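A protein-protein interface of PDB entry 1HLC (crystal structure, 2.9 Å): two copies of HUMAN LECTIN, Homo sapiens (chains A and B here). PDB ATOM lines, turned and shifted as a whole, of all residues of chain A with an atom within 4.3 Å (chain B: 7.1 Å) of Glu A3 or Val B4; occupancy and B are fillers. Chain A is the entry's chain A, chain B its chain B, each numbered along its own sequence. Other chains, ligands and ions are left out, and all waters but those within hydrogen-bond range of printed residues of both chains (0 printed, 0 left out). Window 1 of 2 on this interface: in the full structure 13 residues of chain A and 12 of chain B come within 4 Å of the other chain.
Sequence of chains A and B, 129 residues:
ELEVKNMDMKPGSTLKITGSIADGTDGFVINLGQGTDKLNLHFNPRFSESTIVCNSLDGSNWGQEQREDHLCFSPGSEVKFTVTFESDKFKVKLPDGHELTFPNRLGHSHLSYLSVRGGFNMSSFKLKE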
ATOM      1  N   GLU A   1      -7.953  23.581 -20.949  1.00  0.00           N
ATOM      2  CA  GLU A   1      -6.564  23.112 -20.662  1.00  0.00           C
ATOM      3  C   GLU A   1      -5.534  23.788 -21.590  1.00  0.00           C
ATOM      4  O   GLU A   1      -4.330  23.549 -21.472  1.00  0.00           O
ATOM      5  CB  GLU A   1      -6.495  21.585 -20.808  1.00  0.00           C
ATOM      6  CG  GLU A   1      -5.191  20.958 -20.303  1.00  0.00           C
ATOM      7  CD  GLU A   1      -4.991  19.503 -20.750  1.00  0.00           C
ATOM      8  OE1 GLU A   1      -5.720  19.036 -21.669  1.00  0.00           O
ATOM      9  OE2 GLU A   1      -4.083  18.839 -20.184  1.00  0.00           O
ATOM     10  N   LEU A   2      -6.016  24.635 -22.502  1.00  0.00           N
ATOM     11  CA  LEU A   2      -5.151  25.328 -23.450  1.00  0.00           C
ATOM     12  C   LEU A   2      -4.109  26.162 -22.719  1.00  0.00           C
ATOM     13  O   LEU A   2      -4.380  26.692 -21.635  1.00  0.00           O
ATOM     14  CB  LEU A   2      -5.988  26.197 -24.394  1.00  0.00           C
ATOM     15  CG  LEU A   2      -5.234  26.961 -25.482  1.00  0.00           C
ATOM     16  CD1 LEU A   2      -6.116  27.151 -26.696  1.00  0.00           C
ATOM     17  CD2 LEU A   2      -4.761  28.290 -24.956  1.00  0.00           C
ATOM     18  N   GLU A   3      -2.935  26.298 -23.328  1.00  0.00           N
ATOM     19  CA  GLU A   3      -1.852  27.047 -22.723  1.00  0.00           C
ATOM     20  C   GLU A   3      -0.937  27.799 -23.680  1.00  0.00           C
ATOM     21  O   GLU A   3      -0.091  27.194 -24.327  1.00  0.00           O
ATOM     22  CB  GLU A   3      -0.991  26.119 -21.878  1.00  0.00           C
ATOM     23  CG  GLU A   3       0.201  26.825 -21.277  1.00  0.00           C
ATOM     24  CD  GLU A   3       1.189  25.870 -20.670  1.00  0.00           C
ATOM     25  OE1 GLU A   3       0.865  25.270 -19.621  1.00  0.00           O
ATOM     26  OE2 GLU A   3       2.289  25.710 -21.247  1.00  0.00           O
ATOM     27  N   VAL A   4      -1.086  29.114 -23.750  1.00  0.00           N
ATOM     28  CA  VAL A   4      -0.230  29.922 -24.589  1.00  0.00           C
ATOM     29  C   VAL A   4       1.023  30.133 -23.756  1.00  0.00           C
ATOM     30  O   VAL A   4       0.927  30.385 -22.564  1.00  0.00           O
ATOM     31  CB  VAL A   4      -0.871  31.251 -24.896  1.00  0.00           C
ATOM     32  CG1 VAL A   4       0.123  32.150 -25.607  1.00  0.00           C
ATOM     33  CG2 VAL A   4      -2.098  31.038 -25.740  1.00  0.00           C
ATOM     34  N   LYS A   5       2.192  30.073 -24.378  1.00  0.00           N
ATOM     35  CA  LYS A   5       3.455  30.193 -23.651  1.00  0.00           C
ATOM     36  C   LYS A   5       4.421  31.082 -24.386  1.00  0.00           C
ATOM     37  O   LYS A   5       4.505  31.037 -25.601  1.00  0.00           O
ATOM     38  CB  LYS A   5       4.073  28.802 -23.550  1.00  0.00           C
ATOM     39  CG  LYS A   5       4.971  28.513 -22.372  1.00  0.00           C
ATOM     40  CD  LYS A   5       5.194  26.998 -22.352  1.00  0.00           C
ATOM     41  CE  LYS A   5       5.867  26.483 -21.087  1.00  0.00           C
ATOM     42  NZ  LYS A   5       5.809  24.977 -21.008  1.00  0.00           N
ATOM     43  N   TYR A 113       2.783  34.199 -19.921  1.00  0.00           N
ATOM     44  CA  TYR A 113       2.054  32.939 -19.881  1.00  0.00           C
ATOM     45  C   TYR A 113       0.565  33.221 -19.665  1.00  0.00           C
ATOM     46  O   TYR A 113       0.195  34.163 -18.957  1.00  0.00           O
ATOM     47  CB  TYR A 113       2.636  32.087 -18.743  1.00  0.00           C
ATOM     48  CG  TYR A 113       1.852  30.859 -18.360  1.00  0.00           C
ATOM     49  CD1 TYR A 113       0.859  30.924 -17.386  1.00  0.00           C
ATOM     50  CD2 TYR A 113       2.145  29.622 -18.926  1.00  0.00           C
ATOM     51  CE1 TYR A 113       0.193  29.793 -16.984  1.00  0.00           C
ATOM     52  CE2 TYR A 113       1.489  28.483 -18.533  1.00  0.00           C
ATOM     53  CZ  TYR A 113       0.512  28.570 -17.563  1.00  0.00           C
ATOM     54  OH  TYR A 113      -0.153  27.433 -17.165  1.00  0.00           O
ATOM     55  N   LEU A 114      -0.276  32.417 -20.304  1.00  0.00           N
ATOM     56  CA  LEU A 114      -1.731  32.533 -20.211  1.00  0.00           C
ATOM     57  C   LEU A 114      -2.208  31.093 -20.245  1.00  0.00           C
ATOM     58  O   LEU A 114      -1.598  30.267 -20.910  1.00  0.00           O
ATOM     59  CB  LEU A 114      -2.282  33.275 -21.442  1.00  0.00           C
ATOM     60  CG  LEU A 114      -3.734  33.752 -21.628  1.00  0.00           C
ATOM     61  CD1 LEU A 114      -3.976  33.971 -23.100  1.00  0.00           C
ATOM     62  CD2 LEU A 114      -4.746  32.774 -21.130  1.00  0.00           C
ATOM     63  N   GLU B   1      10.080  31.263 -29.431  1.00  0.00           N
ATOM     64  CA  GLU B   1       9.670  30.247 -28.424  1.00  0.00           C
ATOM     65  C   GLU B   1       8.169  30.261 -28.081  1.00  0.00           C
ATOM     66  O   GLU B   1       7.708  29.437 -27.287  1.00  0.00           O
ATOM     67  CB  GLU B   1      10.525  30.377 -27.156  1.00  0.00           C
ATOM     68  CG  GLU B   1      11.813  29.554 -27.179  1.00  0.00           C
ATOM     69  CD  GLU B   1      11.600  28.055 -26.891  1.00  0.00           C
ATOM     70  OE1 GLU B   1      10.463  27.533 -27.077  1.00  0.00           O
ATOM     71  OE2 GLU B   1      12.585  27.390 -26.473  1.00  0.00           O
ATOM     72  N   LEU B   2       7.406  31.178 -28.677  1.00  0.00           N
ATOM     73  CA  LEU B   2       5.975  31.227 -28.428  1.00  0.00           C
ATOM     74  C   LEU B   2       5.378  29.895 -28.844  1.00  0.00           C
ATOM     75  O   LEU B   2       5.696  29.374 -29.919  1.00  0.00           O
ATOM     76  CB  LEU B   2       5.307  32.332 -29.249  1.00  0.00           C
ATOM     77  CG  LEU B   2       3.769  32.339 -29.208  1.00  0.00           C
ATOM     78  CD1 LEU B   2       3.271  33.105 -27.993  1.00  0.00           C
ATOM     79  CD2 LEU B   2       3.230  32.980 -30.462  1.00  0.00           C
ATOM     80  N   GLU B   3       4.520  29.341 -27.996  1.00  0.00           N
ATOM     81  CA  GLU B   3       3.869  28.079 -28.307  1.00  0.00           C
ATOM     82  C   GLU B   3       2.500  27.960 -27.681  1.00  0.00           C
ATOM     83  O   GLU B   3       2.322  28.299 -26.517  1.00  0.00           O
ATOM     84  CB  GLU B   3       4.756  26.881 -27.937  1.00  0.00           C
ATOM     85  CG  GLU B   3       5.270  26.822 -26.514  1.00  0.00           C
ATOM     86  CD  GLU B   3       6.377  25.786 -26.342  1.00  0.00           C
ATOM     87  OE1 GLU B   3       6.736  25.114 -27.326  1.00  0.00           O
ATOM     88  OE2 GLU B   3       6.896  25.638 -25.216  1.00  0.00           O
ATOM     89  N   VAL B   4       1.527  27.561 -28.498  1.00  0.00           N
ATOM     90  CA  VAL B   4       0.148  27.367 -28.066  1.00  0.00           C
ATOM     91  C   VAL B   4      -0.031  25.869 -27.848  1.00  0.00           C
ATOM     92  O   VAL B   4      -0.167  25.109 -28.797  1.00  0.00           O
ATOM     93  CB  VAL B   4      -0.891  27.844 -29.127  1.00  0.00           C
ATOM     94  CG1 VAL B   4      -2.279  27.870 -28.519  1.00  0.00           C
ATOM     95  CG2 VAL B   4      -0.533  29.210 -29.662  1.00  0.00           C
ATOM     96  N   LYS B   5       0.042  25.441 -26.600  1.00  0.00           N
ATOM     97  CA  LYS B   5      -0.107  24.041 -26.271  1.00  0.00           C
ATOM     98  C   LYS B   5      -1.561  23.724 -26.022  1.00  0.00           C
ATOM     99  O   LYS B   5      -2.297  24.555 -25.503  1.00  0.00           O
ATOM    100  CB  LYS B   5       0.685  23.720 -25.010  1.00  0.00           C
ATOM    101  CG  LYS B   5       2.186  23.667 -25.198  1.00  0.00           C
ATOM    102  CD  LYS B   5       2.711  22.269 -24.849  1.00  0.00           C
ATOM    103  CE  LYS B   5       4.203  22.153 -25.084  1.00  0.00           C
ATOM    104  NZ  LYS B   5       4.964  23.125 -24.248  1.00  0.00           N
ATOM    105  N   ASN B   6      -1.984  22.545 -26.451  1.00  0.00           N
ATOM    106  CA  ASN B   6      -3.349  22.085 -26.213  1.00  0.00           C
ATOM    107  C   ASN B   6      -4.550  22.558 -27.038  1.00  0.00           C
ATOM    108  O   ASN B   6      -5.686  22.440 -26.572  1.00  0.00           O
ATOM    109  CB  ASN B   6      -3.689  22.249 -24.735  1.00  0.00           C
ATOM    110  CG  ASN B   6      -3.434  20.998 -23.943  1.00  0.00           C
ATOM    111  OD1 ASN B   6      -3.605  19.879 -24.451  1.00  0.00           O
ATOM    112  ND2 ASN B   6      -3.032  21.167 -22.682  1.00  0.00           N
ATOM    113  N   MET B   7      -4.347  23.054 -28.255  1.00  0.00           N
ATOM    114  CA  MET B   7      -5.502  23.490 -29.037  1.00  0.00           C
ATOM    115  C   MET B   7      -6.266  22.296 -29.614  1.00  0.00           C
ATOM    116  O   MET B   7      -5.764  21.165 -29.631  1.00  0.00           O
ATOM    117  CB  MET B   7      -5.126  24.516 -30.114  1.00  0.00           C
ATOM    118  CG  MET B   7      -3.792  24.320 -30.749  1.00  0.00           C
ATOM    119  SD  MET B   7      -3.602  25.401 -32.140  1.00  0.00           S
ATOM    120  CE  MET B   7      -3.562  24.223 -33.429  1.00  0.00           C
ATOM    121  N   SER B 112      -2.684  19.850 -32.356  1.00  0.00           N
ATOM    122  CA  SER B 112      -2.819  20.440 -31.033  1.00  0.00           C
ATOM    123  C   SER B 112      -1.687  21.334 -30.591  1.00  0.00           C
ATOM    124  O   SER B 112      -1.730  21.846 -29.475  1.00  0.00           O
ATOM    125  CB  SER B 112      -3.060  19.358 -29.962  1.00  0.00           C
ATOM    126  OG  SER B 112      -2.170  18.255 -30.081  1.00  0.00           O
ATOM    127  N   TYR B 113      -0.715  21.571 -31.471  1.00  0.00           N
ATOM    128  CA  TYR B 113       0.446  22.387 -31.128  1.00  0.00           C
ATOM    129  C   TYR B 113       0.872  23.402 -32.191  1.00  0.00           C
ATOM    130  O   TYR B 113       1.124  23.027 -33.329  1.00  0.00           O
ATOM    131  CB  TYR B 113       1.613  21.446 -30.806  1.00  0.00           C
ATOM    132  CG  TYR B 113       2.956  22.106 -30.556  1.00  0.00           C
ATOM    133  CD1 TYR B 113       3.325  22.524 -29.280  1.00  0.00           C
ATOM    134  CD2 TYR B 113       3.855  22.304 -31.594  1.00  0.00           C
ATOM    135  CE1 TYR B 113       4.554  23.124 -29.049  1.00  0.00           C
ATOM    136  CE2 TYR B 113       5.072  22.898 -31.374  1.00  0.00           C
ATOM    137  CZ  TYR B 113       5.420  23.310 -30.100  1.00  0.00           C
ATOM    138  OH  TYR B 113       6.636  23.925 -29.901  1.00  0.00           O
ATOM    139  N   LEU B 114       0.908  24.683 -31.823  1.00  0.00           N
ATOM    140  CA  LEU B 114       1.355  25.759 -32.714  1.00  0.00           C
ATOM    141  C   LEU B 114       2.607  26.323 -32.080  1.00  0.00           C
ATOM    142  O   LEU B 114       2.713  26.384 -30.863  1.00  0.00           O
ATOM    143  CB  LEU B 114       0.328  26.895 -32.841  1.00  0.00           C
ATOM    144  CG  LEU B 114       0.780  28.103 -33.697  1.00  0.00           C
ATOM    145  CD1 LEU B 114       0.803  27.723 -35.169  1.00  0.00           C
ATOM    146  CD2 LEU B 114      -0.136  29.297 -33.496  1.00  0.00           C
ATOM    147  N   SER B 115       3.528  26.797 -32.896  1.00  0.00           N
ATOM    148  CA  SER B 115       4.776  27.329 -32.378  1.00  0.00           C
ATOM    149  C   SER B 115       5.306  28.353 -33.358  1.00  0.00           C
ATOM    150  O   SER B 115       5.242  28.148 -34.566  1.00  0.00           O
ATOM    151  CB  SER B 115       5.778  26.180 -32.234  1.00  0.00           C
ATOM    152  OG  SER B 115       7.037  26.622 -31.789  1.00  0.00           O
ATOM    153  N   VAL B 116       5.778  29.479 -32.851  1.00  0.00           N
ATOM    154  CA  VAL B 116       6.337  30.491 -33.727  1.00  0.00           C
ATOM    155  C   VAL B 116       7.799  30.792 -33.361  1.00  0.00           C
ATOM    156  O   VAL B 116       8.166  30.994 -32.190  1.00  0.00           O
ATOM    157  CB  VAL B 116       5.471  31.786 -33.767  1.00  0.00           C
ATOM    158  CG1 VAL B 116       6.163  32.856 -34.607  1.00  0.00           C
ATOM    159  CG2 VAL B 116       4.067  31.482 -34.351  1.00  0.00           C
ATOM    160  N   MET B 122       3.308  37.684 -33.208  1.00  0.00           N
ATOM    161  CA  MET B 122       1.885  37.394 -33.388  1.00  0.00           C
ATOM    162  C   MET B 122       0.968  38.243 -32.527  1.00  0.00           C
ATOM    163  O   MET B 122       1.177  38.371 -31.326  1.00  0.00           O
ATOM    164  CB  MET B 122       1.613  35.929 -33.104  1.00  0.00           C
ATOM    165  CG  MET B 122       0.145  35.584 -33.068  1.00  0.00           C
ATOM    166  SD  MET B 122      -0.126  33.993 -32.297  1.00  0.00           S
ATOM    167  CE  MET B 122       0.087  32.873 -33.724  1.00  0.00           C
ATOM    168  N   PHE B 125      -5.076  35.325 -33.161  1.00  0.00           N
ATOM    169  CA  PHE B 125      -5.208  33.898 -33.263  1.00  0.00           C
ATOM    170  C   PHE B 125      -6.709  33.737 -33.175  1.00  0.00           C
ATOM    171  O   PHE B 125      -7.339  34.289 -32.276  1.00  0.00           O
ATOM    172  CB  PHE B 125      -4.524  33.253 -32.062  1.00  0.00           C
ATOM    173  CG  PHE B 125      -4.880  31.814 -31.842  1.00  0.00           C
ATOM    174  CD1 PHE B 125      -6.044  31.465 -31.148  1.00  0.00           C
ATOM    175  CD2 PHE B 125      -4.020  30.801 -32.246  1.00  0.00           C
ATOM    176  CE1 PHE B 125      -6.346  30.125 -30.850  1.00  0.00           C
ATOM    177  CE2 PHE B 125      -4.311  29.464 -31.954  1.00  0.00           C
ATOM    178  CZ  PHE B 125      -5.483  29.130 -31.249  1.00  0.00           C
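Among the printed residues, pairs that only touch across the chains: Leu A2 with Lys B5 (3.6 Å), Leu A2 with Asn B6 (3.6 Å), Glu A3 with Val B4 (3.8 Å), Val A4 with Glu B3 (3.6 Å), Lys A5 with Glu B1 (3.96 Å), Lys A5 with Leu B2 (3.2 Å) and Lys A5 with Lys B5 (3.8 Å).
Of the 7 printed residues of chain A, 5 touch a printed residue of chain B. Printed residues of chain A that touch a printed residue of chain B: Glu A1, Leu A2, Glu A3, Val A4 and Lys A5. Along chain A the printed residues that touch a printed residue of chain B span positions 1 to 5. Hydrophobic or aromatic side chains of chain B that line the printed part of chain A: Leu B2. Among the printed residues, 11 pairs touch across the chains. Among the printed residues, no Asp or Glu carboxylate lies within 4 Å of a Lys or Arg side-chain nitrogen of the other chain.
Leu A2 touches Lys B5, and with the chains exchanged Lys A5 touches Leu B2. Glu A3 touches Val B4, and with the chains exchanged Val A4 touches Glu B3. Glu A3 touches Lys B5, and with the chains exchanged Lys A5 touches Glu B3. Lys B5 touches its own counterpart, Lys A5. Positions printed for both chains: 1, 2, 3, 4, 5, 113 and 114. Of the 11 pairs that touch across the chains among the printed residues, 8 have their exchanged pair printed and touching as well.
Glu A3 touches just these residues of chain B: Glu B3 (3.4 Å), Val B4 (3.8 Å) and Lys B5 (2.9 Å). Printed residues of chain B within 4 Å of Val A4: Glu B3 (3.6 Å). Of the printed residues of chain A, Glu B1 touches Lys A5. Of the printed residues of chain A, Leu B2 touches Lys A5. Of the printed residues of chain A, Glu B3 touches Glu A3, Val A4 and Lys A5. Of chain A, only Glu A3 comes within 4 Å of Val B4. Met B122 touches none of the printed residues of chain A. The nearest residue of chain B that does not touch Glu A3 is Asn B6 (4.4 Å). The nearest residue of chain A that does not touch Val B4 is Val A4 (4.2 Å). The nearest printed residue of chain A that does not touch Lys B5 is Glu A1 (4.6 Å).
The side-chain carboxylate (OE1) of Glu B3 is in hydrogen-bond range of the side-chain hydroxyl (OH) of Tyr B113. O of Ser B112 is in hydrogen-bond range of N of Asn B6 (3.1 Å). The backbone carbonyl oxygen of Leu B114 sits at hydrogen-bond distance from the backbone NH of Val B4 (2.9 Å). The backbone carbonyl oxygen of Val B116 is in hydrogen-bond range of the backbone NH of Glu B1 (3.4 Å). NZ of Lys A5 is in salt-bridge range of OE2 of Glu A3, at 3.6 Å. The backbone NH (N) of Val B116 lies within hydrogen-bond range of the backbone carbonyl oxygen (O) of Leu B2 (2.9 Å).
N of Glu A3 is in hydrogen-bond range of O of Lys B5 (2.9 Å). O of Glu A3 lies close to O of Glu B3. The backbone NH of Lys A5 is in hydrogen-bond range of the backbone carbonyl oxygen of Glu B3, 2.8 Å away. The backbone carbonyl oxygen of Glu A1 sits at hydrogen-bond distance from the side-chain amide nitrogen of Asn B6.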
